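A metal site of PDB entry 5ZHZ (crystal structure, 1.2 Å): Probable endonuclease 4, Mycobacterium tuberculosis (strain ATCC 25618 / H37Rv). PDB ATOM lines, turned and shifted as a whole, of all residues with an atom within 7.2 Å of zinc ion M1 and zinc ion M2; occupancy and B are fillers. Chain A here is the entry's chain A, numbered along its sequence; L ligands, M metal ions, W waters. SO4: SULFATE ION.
N of Asp 162 sits at hydrogen-bond distance from OD1 of Asn 130 (2.9 Å).
The side-chain carboxylate (OD1) of Asp 162 lies within hydrogen-bond range of the backbone NH (N) of Cys 164, 2.9 Å away.
The backbone NH of Glu 129 sits at hydrogen-bond distance from the backbone carbonyl oxygen of Val 95 (2.9 Å).
The backbone carbonyl oxygen of Leu 161 lies within hydrogen-bond range of the backbone NH of His 191.
The side-chain sulfur (SG) of Cys 160 sits at hydrogen-bond distance from a ring nitrogen (NE2) of His 191 (3.4 Å).
A ring nitrogen (ND1) of His 165 lies close to the side-chain carboxylate (OE2) of Glu 129 (3.4 Å).
OD1 of Asp 162 sits at hydrogen-bond distance from N of His 165.
A ring nitrogen (ND1) of His 206 sits at hydrogen-bond distance from the backbone carbonyl oxygen (O) of Glu 233, at 2.8 Å.
The side-chain carboxylate (OD2) of Asp 162 is bound to zinc ion M1, at 2.1 Å.
OE2 of Glu 129 is bound to zinc ion M1 (2.1 Å).
Zinc ion M1 is bound by water W1, at 2.1 Å.
OE1 of Glu 233 is bound to zinc ion M1 (2.1 Å).
O2 of the ligand is bound to zinc ion M1.
Zinc ion M1 is bound by ND1 of His 191 (2.2 Å).
Merely in contact with zinc ion M1: His 165 (3.8 Å).
Within 4 Å of zinc ion M1: Glu 129, Asp 162, His 165, His 191 and Glu 233.
Along chain A the residues within 4 Å of zinc ion M1 span positions 129 to 233.
Of the 25 residues printed, 3 come within 4 Å of zinc ion M2.
The nearest printed residue that does not touch zinc ion M2 is His 191 (4.2 Å).
Zinc ion M2 is bound by a ring nitrogen (NE2) of His 96, water W1, the side-chain carboxylate of Glu 129, a ring nitrogen (NE2) of His 56 and an oxygen (O3) of the ligand.
Zinc ion M2 has five donor atoms within binding distance.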
ATOM      1  N   GLN A  25      20.493  20.816  15.689  1.00  0.00           N
ATOM      2  CA  GLN A  25      20.122  21.874  14.767  1.00  0.00           C
ATOM      3  C   GLN A  25      19.663  23.072  15.605  1.00  0.00           C
ATOM      4  O   GLN A  25      18.993  22.889  16.632  1.00  0.00           O
ATOM      5  CB  GLN A  25      19.008  21.395  13.860  1.00  0.00           C
ATOM      6  CG  GLN A  25      18.589  22.377  12.767  1.00  0.00           C
ATOM      7  CD  GLN A  25      17.486  21.784  11.950  1.00  0.00           C
ATOM      8  OE1 GLN A  25      17.735  21.111  10.921  1.00  0.00           O
ATOM      9  NE2 GLN A  25      16.234  21.960  12.398  1.00  0.00           N
ATOM     10  N   PHE A  27      18.534  27.548  15.367  1.00  0.00           N
ATOM     11  CA  PHE A  27      18.442  28.859  14.733  1.00  0.00           C
ATOM     12  C   PHE A  27      19.522  29.760  15.282  1.00  0.00           C
ATOM     13  O   PHE A  27      19.929  29.678  16.440  1.00  0.00           O
ATOM     14  CB  PHE A  27      17.085  29.515  15.006  1.00  0.00           C
ATOM     15  CG  PHE A  27      15.929  28.858  14.270  1.00  0.00           C
ATOM     16  CD1 PHE A  27      15.615  29.296  12.989  1.00  0.00           C
ATOM     17  CD2 PHE A  27      15.221  27.819  14.815  1.00  0.00           C
ATOM     18  CE1 PHE A  27      14.570  28.742  12.280  1.00  0.00           C
ATOM     19  CE2 PHE A  27      14.152  27.258  14.062  1.00  0.00           C
ATOM     20  CZ  PHE A  27      13.874  27.710  12.815  1.00  0.00           C
ATOM     21  N   HIS A  56      19.107  26.125  10.937  1.00  0.00           N
ATOM     22  CA  HIS A  56      17.861  26.393  10.247  1.00  0.00           C
ATOM     23  C   HIS A  56      17.770  27.869   9.898  1.00  0.00           C
ATOM     24  O   HIS A  56      17.922  28.715  10.788  1.00  0.00           O
ATOM     25  CB  HIS A  56      16.674  25.969  11.134  1.00  0.00           C
ATOM     26  CG  HIS A  56      15.401  25.738  10.379  1.00  0.00           C
ATOM     27  ND1 HIS A  56      14.821  26.691   9.546  1.00  0.00           N
ATOM     28  CD2 HIS A  56      14.597  24.648  10.306  1.00  0.00           C
ATOM     29  CE1 HIS A  56      13.731  26.167   9.003  1.00  0.00           C
ATOM     30  NE2 HIS A  56      13.552  24.935   9.455  1.00  0.00           N
ATOM     31  N   ALA A  57      17.568  28.196   8.625  1.00  0.00           N
ATOM     32  CA  ALA A  57      17.428  29.581   8.232  1.00  0.00           C
ATOM     33  C   ALA A  57      16.076  30.125   8.721  1.00  0.00           C
ATOM     34  O   ALA A  57      15.125  29.360   8.889  1.00  0.00           O
ATOM     35  CB  ALA A  57      17.495  29.687   6.711  1.00  0.00           C
ATOM     36  N   TYR A  59      12.367  31.406   9.287  1.00  0.00           N
ATOM     37  CA  TYR A  59      11.155  30.882   8.666  1.00  0.00           C
ATOM     38  C   TYR A  59      10.556  31.812   7.627  1.00  0.00           C
ATOM     39  O   TYR A  59       9.848  31.340   6.727  1.00  0.00           O
ATOM     40  CB  TYR A  59      10.095  30.733   9.723  1.00  0.00           C
ATOM     41  CG  TYR A  59      10.276  29.533  10.603  1.00  0.00           C
ATOM     42  CD1 TYR A  59      10.524  28.245  10.052  1.00  0.00           C
ATOM     43  CD2 TYR A  59      10.197  29.634  11.988  1.00  0.00           C
ATOM     44  CE1 TYR A  59      10.647  27.122  10.867  1.00  0.00           C
ATOM     45  CE2 TYR A  59      10.344  28.497  12.792  1.00  0.00           C
ATOM     46  CZ  TYR A  59      10.534  27.266  12.232  1.00  0.00           C
ATOM     47  OH  TYR A  59      10.664  26.184  13.064  1.00  0.00           O
ATOM     48  N   ILE A  94      19.456  24.818   6.465  1.00  0.00           N
ATOM     49  CA  ILE A  94      18.179  24.309   5.984  1.00  0.00           C
ATOM     50  C   ILE A  94      17.247  25.486   5.739  1.00  0.00           C
ATOM     51  O   ILE A  94      17.101  26.358   6.595  1.00  0.00           O
ATOM     52  CB  ILE A  94      17.573  23.352   7.038  1.00  0.00           C
ATOM     53  CG1 ILE A  94      18.412  22.083   7.225  1.00  0.00           C
ATOM     54  CG2 ILE A  94      16.176  22.906   6.596  1.00  0.00           C
ATOM     55  CD1 ILE A  94      19.639  22.249   8.048  1.00  0.00           C
ATOM     56  N   VAL A  95      16.587  25.497   4.583  1.00  0.00           N
ATOM     57  CA  VAL A  95      15.648  26.575   4.261  1.00  0.00           C
ATOM     58  C   VAL A  95      14.380  25.962   3.687  1.00  0.00           C
ATOM     59  O   VAL A  95      14.424  25.017   2.894  1.00  0.00           O
ATOM     60  CB  VAL A  95      16.299  27.596   3.306  1.00  0.00           C
ATOM     61  CG1 VAL A  95      16.675  26.983   2.037  1.00  0.00           C
ATOM     62  CG2 VAL A  95      15.381  28.767   3.045  1.00  0.00           C
ATOM     63  N   HIS A  96      13.236  26.485   4.085  1.00  0.00           N
ATOM     64  CA  HIS A  96      11.966  26.004   3.582  1.00  0.00           C
ATOM     65  C   HIS A  96      11.770  26.365   2.112  1.00  0.00           C
ATOM     66  O   HIS A  96      12.319  27.347   1.591  1.00  0.00           O
ATOM     67  CB  HIS A  96      10.853  26.528   4.464  1.00  0.00           C
ATOM     68  CG  HIS A  96      10.834  25.839   5.890  1.00  0.00           C
ATOM     69  ND1 HIS A  96       9.706  26.071   6.598  1.00  0.00           N
ATOM     70  CD2 HIS A  96      11.619  24.929   6.761  1.00  0.00           C
ATOM     71  CE1 HIS A  96       9.841  25.444   7.758  1.00  0.00           C
ATOM     72  NE2 HIS A  96      10.954  24.762   7.806  1.00  0.00           N
ATOM     73  N   GLU A 129      13.850  22.213   2.515  1.00  0.00           N
ATOM     74  CA  GLU A 129      12.948  21.380   3.300  1.00  0.00           C
ATOM     75  C   GLU A 129      11.506  21.506   2.781  1.00  0.00           C
ATOM     76  O   GLU A 129      11.022  22.611   2.490  1.00  0.00           O
ATOM     77  CB  GLU A 129      13.001  21.837   4.788  1.00  0.00           C
ATOM     78  CG  GLU A 129      12.176  20.940   5.719  1.00  0.00           C
ATOM     79  CD  GLU A 129      12.039  21.452   7.156  1.00  0.00           C
ATOM     80  OE1 GLU A 129      12.737  22.452   7.473  1.00  0.00           O
ATOM     81  OE2 GLU A 129      11.232  20.874   7.928  1.00  0.00           O
ATOM     82  N   ASN A 130      10.822  20.365   2.708  1.00  0.00           N
ATOM     83  CA  ASN A 130       9.402  20.365   2.373  1.00  0.00           C
ATOM     84  C   ASN A 130       8.576  20.986   3.492  1.00  0.00           C
ATOM     85  O   ASN A 130       8.989  20.985   4.664  1.00  0.00           O
ATOM     86  CB  ASN A 130       8.889  18.978   2.036  1.00  0.00           C
ATOM     87  CG  ASN A 130       9.029  17.994   3.178  1.00  0.00           C
ATOM     88  OD1 ASN A 130      10.108  17.806   3.722  1.00  0.00           O
ATOM     89  ND2 ASN A 130       7.942  17.308   3.495  1.00  0.00           N
ATOM     90  N   THR A 131       7.368  21.465   3.136  1.00  0.00           N
ATOM     91  CA  THR A 131       6.530  22.235   4.058  1.00  0.00           C
ATOM     92  C   THR A 131       5.155  21.608   4.209  1.00  0.00           C
ATOM     93  O   THR A 131       4.750  20.739   3.453  1.00  0.00           O
ATOM     94  CB  THR A 131       6.439  23.692   3.567  1.00  0.00           C
ATOM     95  OG1 THR A 131       5.944  23.708   2.217  1.00  0.00           O
ATOM     96  CG2 THR A 131       7.804  24.367   3.607  1.00  0.00           C
ATOM     97  N   CYS A 160      16.010  18.177   2.611  1.00  0.00           N
ATOM     98  CA  CYS A 160      15.690  17.739   3.950  1.00  0.00           C
ATOM     99  C   CYS A 160      14.232  17.314   3.984  1.00  0.00           C
ATOM    100  O   CYS A 160      13.333  18.122   3.689  1.00  0.00           O
ATOM    101  CB  CYS A 160      15.902  18.909   4.932  1.00  0.00           C
ATOM    102  SG  CYS A 160      15.337  18.544   6.603  1.00  0.00           S
ATOM    103  N   LEU A 161      13.986  16.048   4.333  1.00  0.00           N
ATOM    104  CA  LEU A 161      12.627  15.521   4.415  1.00  0.00           C
ATOM    105  C   LEU A 161      12.114  15.632   5.848  1.00  0.00           C
ATOM    106  O   LEU A 161      12.712  15.060   6.772  1.00  0.00           O
ATOM    107  CB  LEU A 161      12.611  14.050   3.962  1.00  0.00           C
ATOM    108  CG  LEU A 161      11.204  13.437   4.025  1.00  0.00           C
ATOM    109  CD1 LEU A 161      10.241  14.079   2.998  1.00  0.00           C
ATOM    110  CD2 LEU A 161      11.245  11.931   3.746  1.00  0.00           C
ATOM    111  N   ASP A 162      11.002  16.362   6.044  1.00  0.00           N
ATOM    112  CA  ASP A 162      10.384  16.474   7.352  1.00  0.00           C
ATOM    113  C   ASP A 162       9.144  15.577   7.356  1.00  0.00           C
ATOM    114  O   ASP A 162       8.228  15.740   6.515  1.00  0.00           O
ATOM    115  CB  ASP A 162      10.042  17.929   7.639  1.00  0.00           C
ATOM    116  CG  ASP A 162       9.514  18.139   9.075  1.00  0.00           C
ATOM    117  OD1 ASP A 162       8.524  17.449   9.418  1.00  0.00           O
ATOM    118  OD2 ASP A 162      10.092  18.970   9.794  1.00  0.00           O
ATOM    119  N   THR A 163       9.126  14.602   8.274  1.00  0.00           N
ATOM    120  CA  THR A 163       8.034  13.632   8.286  1.00  0.00           C
ATOM    121  C   THR A 163       6.707  14.239   8.721  1.00  0.00           C
ATOM    122  O   THR A 163       5.651  13.764   8.272  1.00  0.00           O
ATOM    123  CB  THR A 163       8.362  12.434   9.186  1.00  0.00           C
ATOM    124  OG1 THR A 163       8.661  12.903  10.513  1.00  0.00           O
ATOM    125  CG2 THR A 163       9.610  11.693   8.670  1.00  0.00           C
ATOM    126  N   CYS A 164       6.719  15.207   9.636  1.00  0.00           N
ATOM    127  CA  CYS A 164       5.459  15.848  10.008  1.00  0.00           C
ATOM    128  C   CYS A 164       4.893  16.610   8.820  1.00  0.00           C
ATOM    129  O   CYS A 164       3.673  16.580   8.557  1.00  0.00           O
ATOM    130  CB  CYS A 164       5.665  16.769  11.223  1.00  0.00           C
ATOM    131  SG  CYS A 164       4.129  17.615  11.793  1.00  0.00           S
ATOM    132  N   HIS A 165       5.756  17.311   8.093  1.00  0.00           N
ATOM    133  CA  HIS A 165       5.293  18.074   6.942  1.00  0.00           C
ATOM    134  C   HIS A 165       4.708  17.152   5.883  1.00  0.00           C
ATOM    135  O   HIS A 165       3.658  17.451   5.284  1.00  0.00           O
ATOM    136  CB  HIS A 165       6.401  18.976   6.385  1.00  0.00           C
ATOM    137  CG  HIS A 165       6.901  19.945   7.414  1.00  0.00           C
ATOM    138  ND1 HIS A 165       7.943  20.817   7.223  1.00  0.00           N
ATOM    139  CD2 HIS A 165       6.459  20.166   8.695  1.00  0.00           C
ATOM    140  CE1 HIS A 165       8.165  21.497   8.348  1.00  0.00           C
ATOM    141  NE2 HIS A 165       7.267  21.121   9.262  1.00  0.00           N
ATOM    142  N   VAL A 190      17.015  14.166   7.632  1.00  0.00           N
ATOM    143  CA  VAL A 190      15.602  13.901   7.943  1.00  0.00           C
ATOM    144  C   VAL A 190      15.235  14.636   9.210  1.00  0.00           C
ATOM    145  O   VAL A 190      16.003  14.573  10.201  1.00  0.00           O
ATOM    146  CB  VAL A 190      15.335  12.388   8.072  1.00  0.00           C
ATOM    147  CG1 VAL A 190      13.979  12.103   8.675  1.00  0.00           C
ATOM    148  CG2 VAL A 190      15.460  11.731   6.717  1.00  0.00           C
ATOM    149  N   HIS A 191      14.102  15.324   9.191  1.00  0.00           N
ATOM    150  CA  HIS A 191      13.496  15.839  10.412  1.00  0.00           C
ATOM    151  C   HIS A 191      12.445  14.819  10.805  1.00  0.00           C
ATOM    152  O   HIS A 191      11.421  14.669  10.108  1.00  0.00           O
ATOM    153  CB  HIS A 191      12.858  17.198  10.164  1.00  0.00           C
ATOM    154  CG  HIS A 191      13.834  18.300   9.966  1.00  0.00           C
ATOM    155  ND1 HIS A 191      13.442  19.581   9.594  1.00  0.00           N
ATOM    156  CD2 HIS A 191      15.185  18.314  10.098  1.00  0.00           C
ATOM    157  CE1 HIS A 191      14.528  20.337   9.542  1.00  0.00           C
ATOM    158  NE2 HIS A 191      15.599  19.606   9.842  1.00  0.00           N
ATOM    159  N   CYS A 192      12.708  14.075  11.878  1.00  0.00           N
ATOM    160  CA  CYS A 192      11.831  12.997  12.291  1.00  0.00           C
ATOM    161  C   CYS A 192      10.924  13.497  13.415  1.00  0.00           C
ATOM    162  O   CYS A 192      11.302  13.490  14.601  1.00  0.00           O
ATOM    163  CB  CYS A 192      12.616  11.765  12.727  1.00  0.00           C
ATOM    164  SG  CYS A 192      11.532  10.350  13.069  1.00  0.00           S
ATOM    165  N   ASN A 193       9.733  13.912  13.015  1.00  0.00           N
ATOM    166  CA  ASN A 193       8.709  14.519  13.875  1.00  0.00           C
ATOM    167  C   ASN A 193       7.414  13.736  13.773  1.00  0.00           C
ATOM    168  O   ASN A 193       6.990  13.386  12.678  1.00  0.00           O
ATOM    169  CB  ASN A 193       8.449  15.948  13.379  1.00  0.00           C
ATOM    170  CG  ASN A 193       9.673  16.802  13.425  1.00  0.00           C
ATOM    171  OD1 ASN A 193      10.456  16.725  14.384  1.00  0.00           O
ATOM    172  ND2 ASN A 193       9.876  17.618  12.379  1.00  0.00           N
ATOM    173  N   ASP A 204       0.892  22.387  11.155  1.00  0.00           N
ATOM    174  CA  ASP A 204       2.275  21.988  11.461  1.00  0.00           C
ATOM    175  C   ASP A 204       2.477  22.037  12.960  1.00  0.00           C
ATOM    176  O   ASP A 204       2.956  23.061  13.506  1.00  0.00           O
ATOM    177  CB  ASP A 204       3.242  22.834  10.804  1.00  0.00           C
ATOM    178  CG  ASP A 204       4.658  22.264  11.048  1.00  0.00           C
ATOM    179  OD1 ASP A 204       4.818  21.044  11.045  1.00  0.00           O
ATOM    180  OD2 ASP A 204       5.622  22.983  11.191  1.00  0.00           O
ATOM    181  N   HIS A 206       4.251  19.770  15.664  1.00  0.00           N
ATOM    182  CA  HIS A 206       5.070  18.577  15.900  1.00  0.00           C
ATOM    183  C   HIS A 206       4.677  17.931  17.212  1.00  0.00           C
ATOM    184  O   HIS A 206       4.178  18.581  18.131  1.00  0.00           O
ATOM    185  CB  HIS A 206       6.554  18.945  15.945  1.00  0.00           C
ATOM    186  CG  HIS A 206       7.076  19.618  14.689  1.00  0.00           C
ATOM    187  ND1 HIS A 206       8.405  19.929  14.548  1.00  0.00           N
ATOM    188  CD2 HIS A 206       6.480  20.068  13.542  1.00  0.00           C
ATOM    189  CE1 HIS A 206       8.604  20.518  13.377  1.00  0.00           C
ATOM    190  NE2 HIS A 206       7.445  20.633  12.725  1.00  0.00           N
ATOM    191  N   ILE A 231      17.260  14.791  12.745  1.00  0.00           N
ATOM    192  CA  ILE A 231      16.936  15.798  13.749  1.00  0.00           C
ATOM    193  C   ILE A 231      15.506  15.561  14.210  1.00  0.00           C
ATOM    194  O   ILE A 231      14.568  15.640  13.401  1.00  0.00           O
ATOM    195  CB  ILE A 231      17.028  17.219  13.187  1.00  0.00           C
ATOM    196  CG1 ILE A 231      18.294  17.525  12.410  1.00  0.00           C
ATOM    197  CG2 ILE A 231      16.752  18.240  14.278  1.00  0.00           C
ATOM    198  CD1 ILE A 231      19.479  17.352  13.143  1.00  0.00           C
ATOM    199  N   GLU A 233      12.641  17.410  15.906  1.00  0.00           N
ATOM    200  CA  GLU A 233      12.263  18.794  16.179  1.00  0.00           C
ATOM    201  C   GLU A 233      11.027  18.791  17.066  1.00  0.00           C
ATOM    202  O   GLU A 233       9.972  19.353  16.776  1.00  0.00           O
ATOM    203  CB  GLU A 233      11.984  19.561  14.875  1.00  0.00           C
ATOM    204  CG  GLU A 233      13.124  19.500  13.886  1.00  0.00           C
ATOM    205  CD  GLU A 233      12.786  20.218  12.626  1.00  0.00           C
ATOM    206  OE1 GLU A 233      11.814  19.843  11.951  1.00  0.00           O
ATOM    207  OE2 GLU A 233      13.442  21.220  12.318  1.00  0.00           O
HETATM  208  S   SO4 L   1       9.840  23.085  11.183  1.00  0.00           S
HETATM  209  O1  SO4 L   1      10.528  23.417  12.445  1.00  0.00           O
HETATM  210  O2  SO4 L   1       9.889  21.627  10.858  1.00  0.00           O
HETATM  211  O3  SO4 L   1      10.274  23.911  10.056  1.00  0.00           O
HETATM  212  O4  SO4 L   1       8.376  23.330  11.345  1.00  0.00           O
HETATM  213 ZN    ZN M   1      11.484  20.489   9.944  1.00  0.00          ZN
HETATM  214 ZN    ZN M   2      12.045  23.616   8.949  1.00  0.00          ZN
HETATM  215 ZN    ZN M   3       7.192  21.770  11.127  1.00  0.00          ZN
HETATM  216  O   HOH W   1      12.566  22.254  10.274  1.00  0.00           O
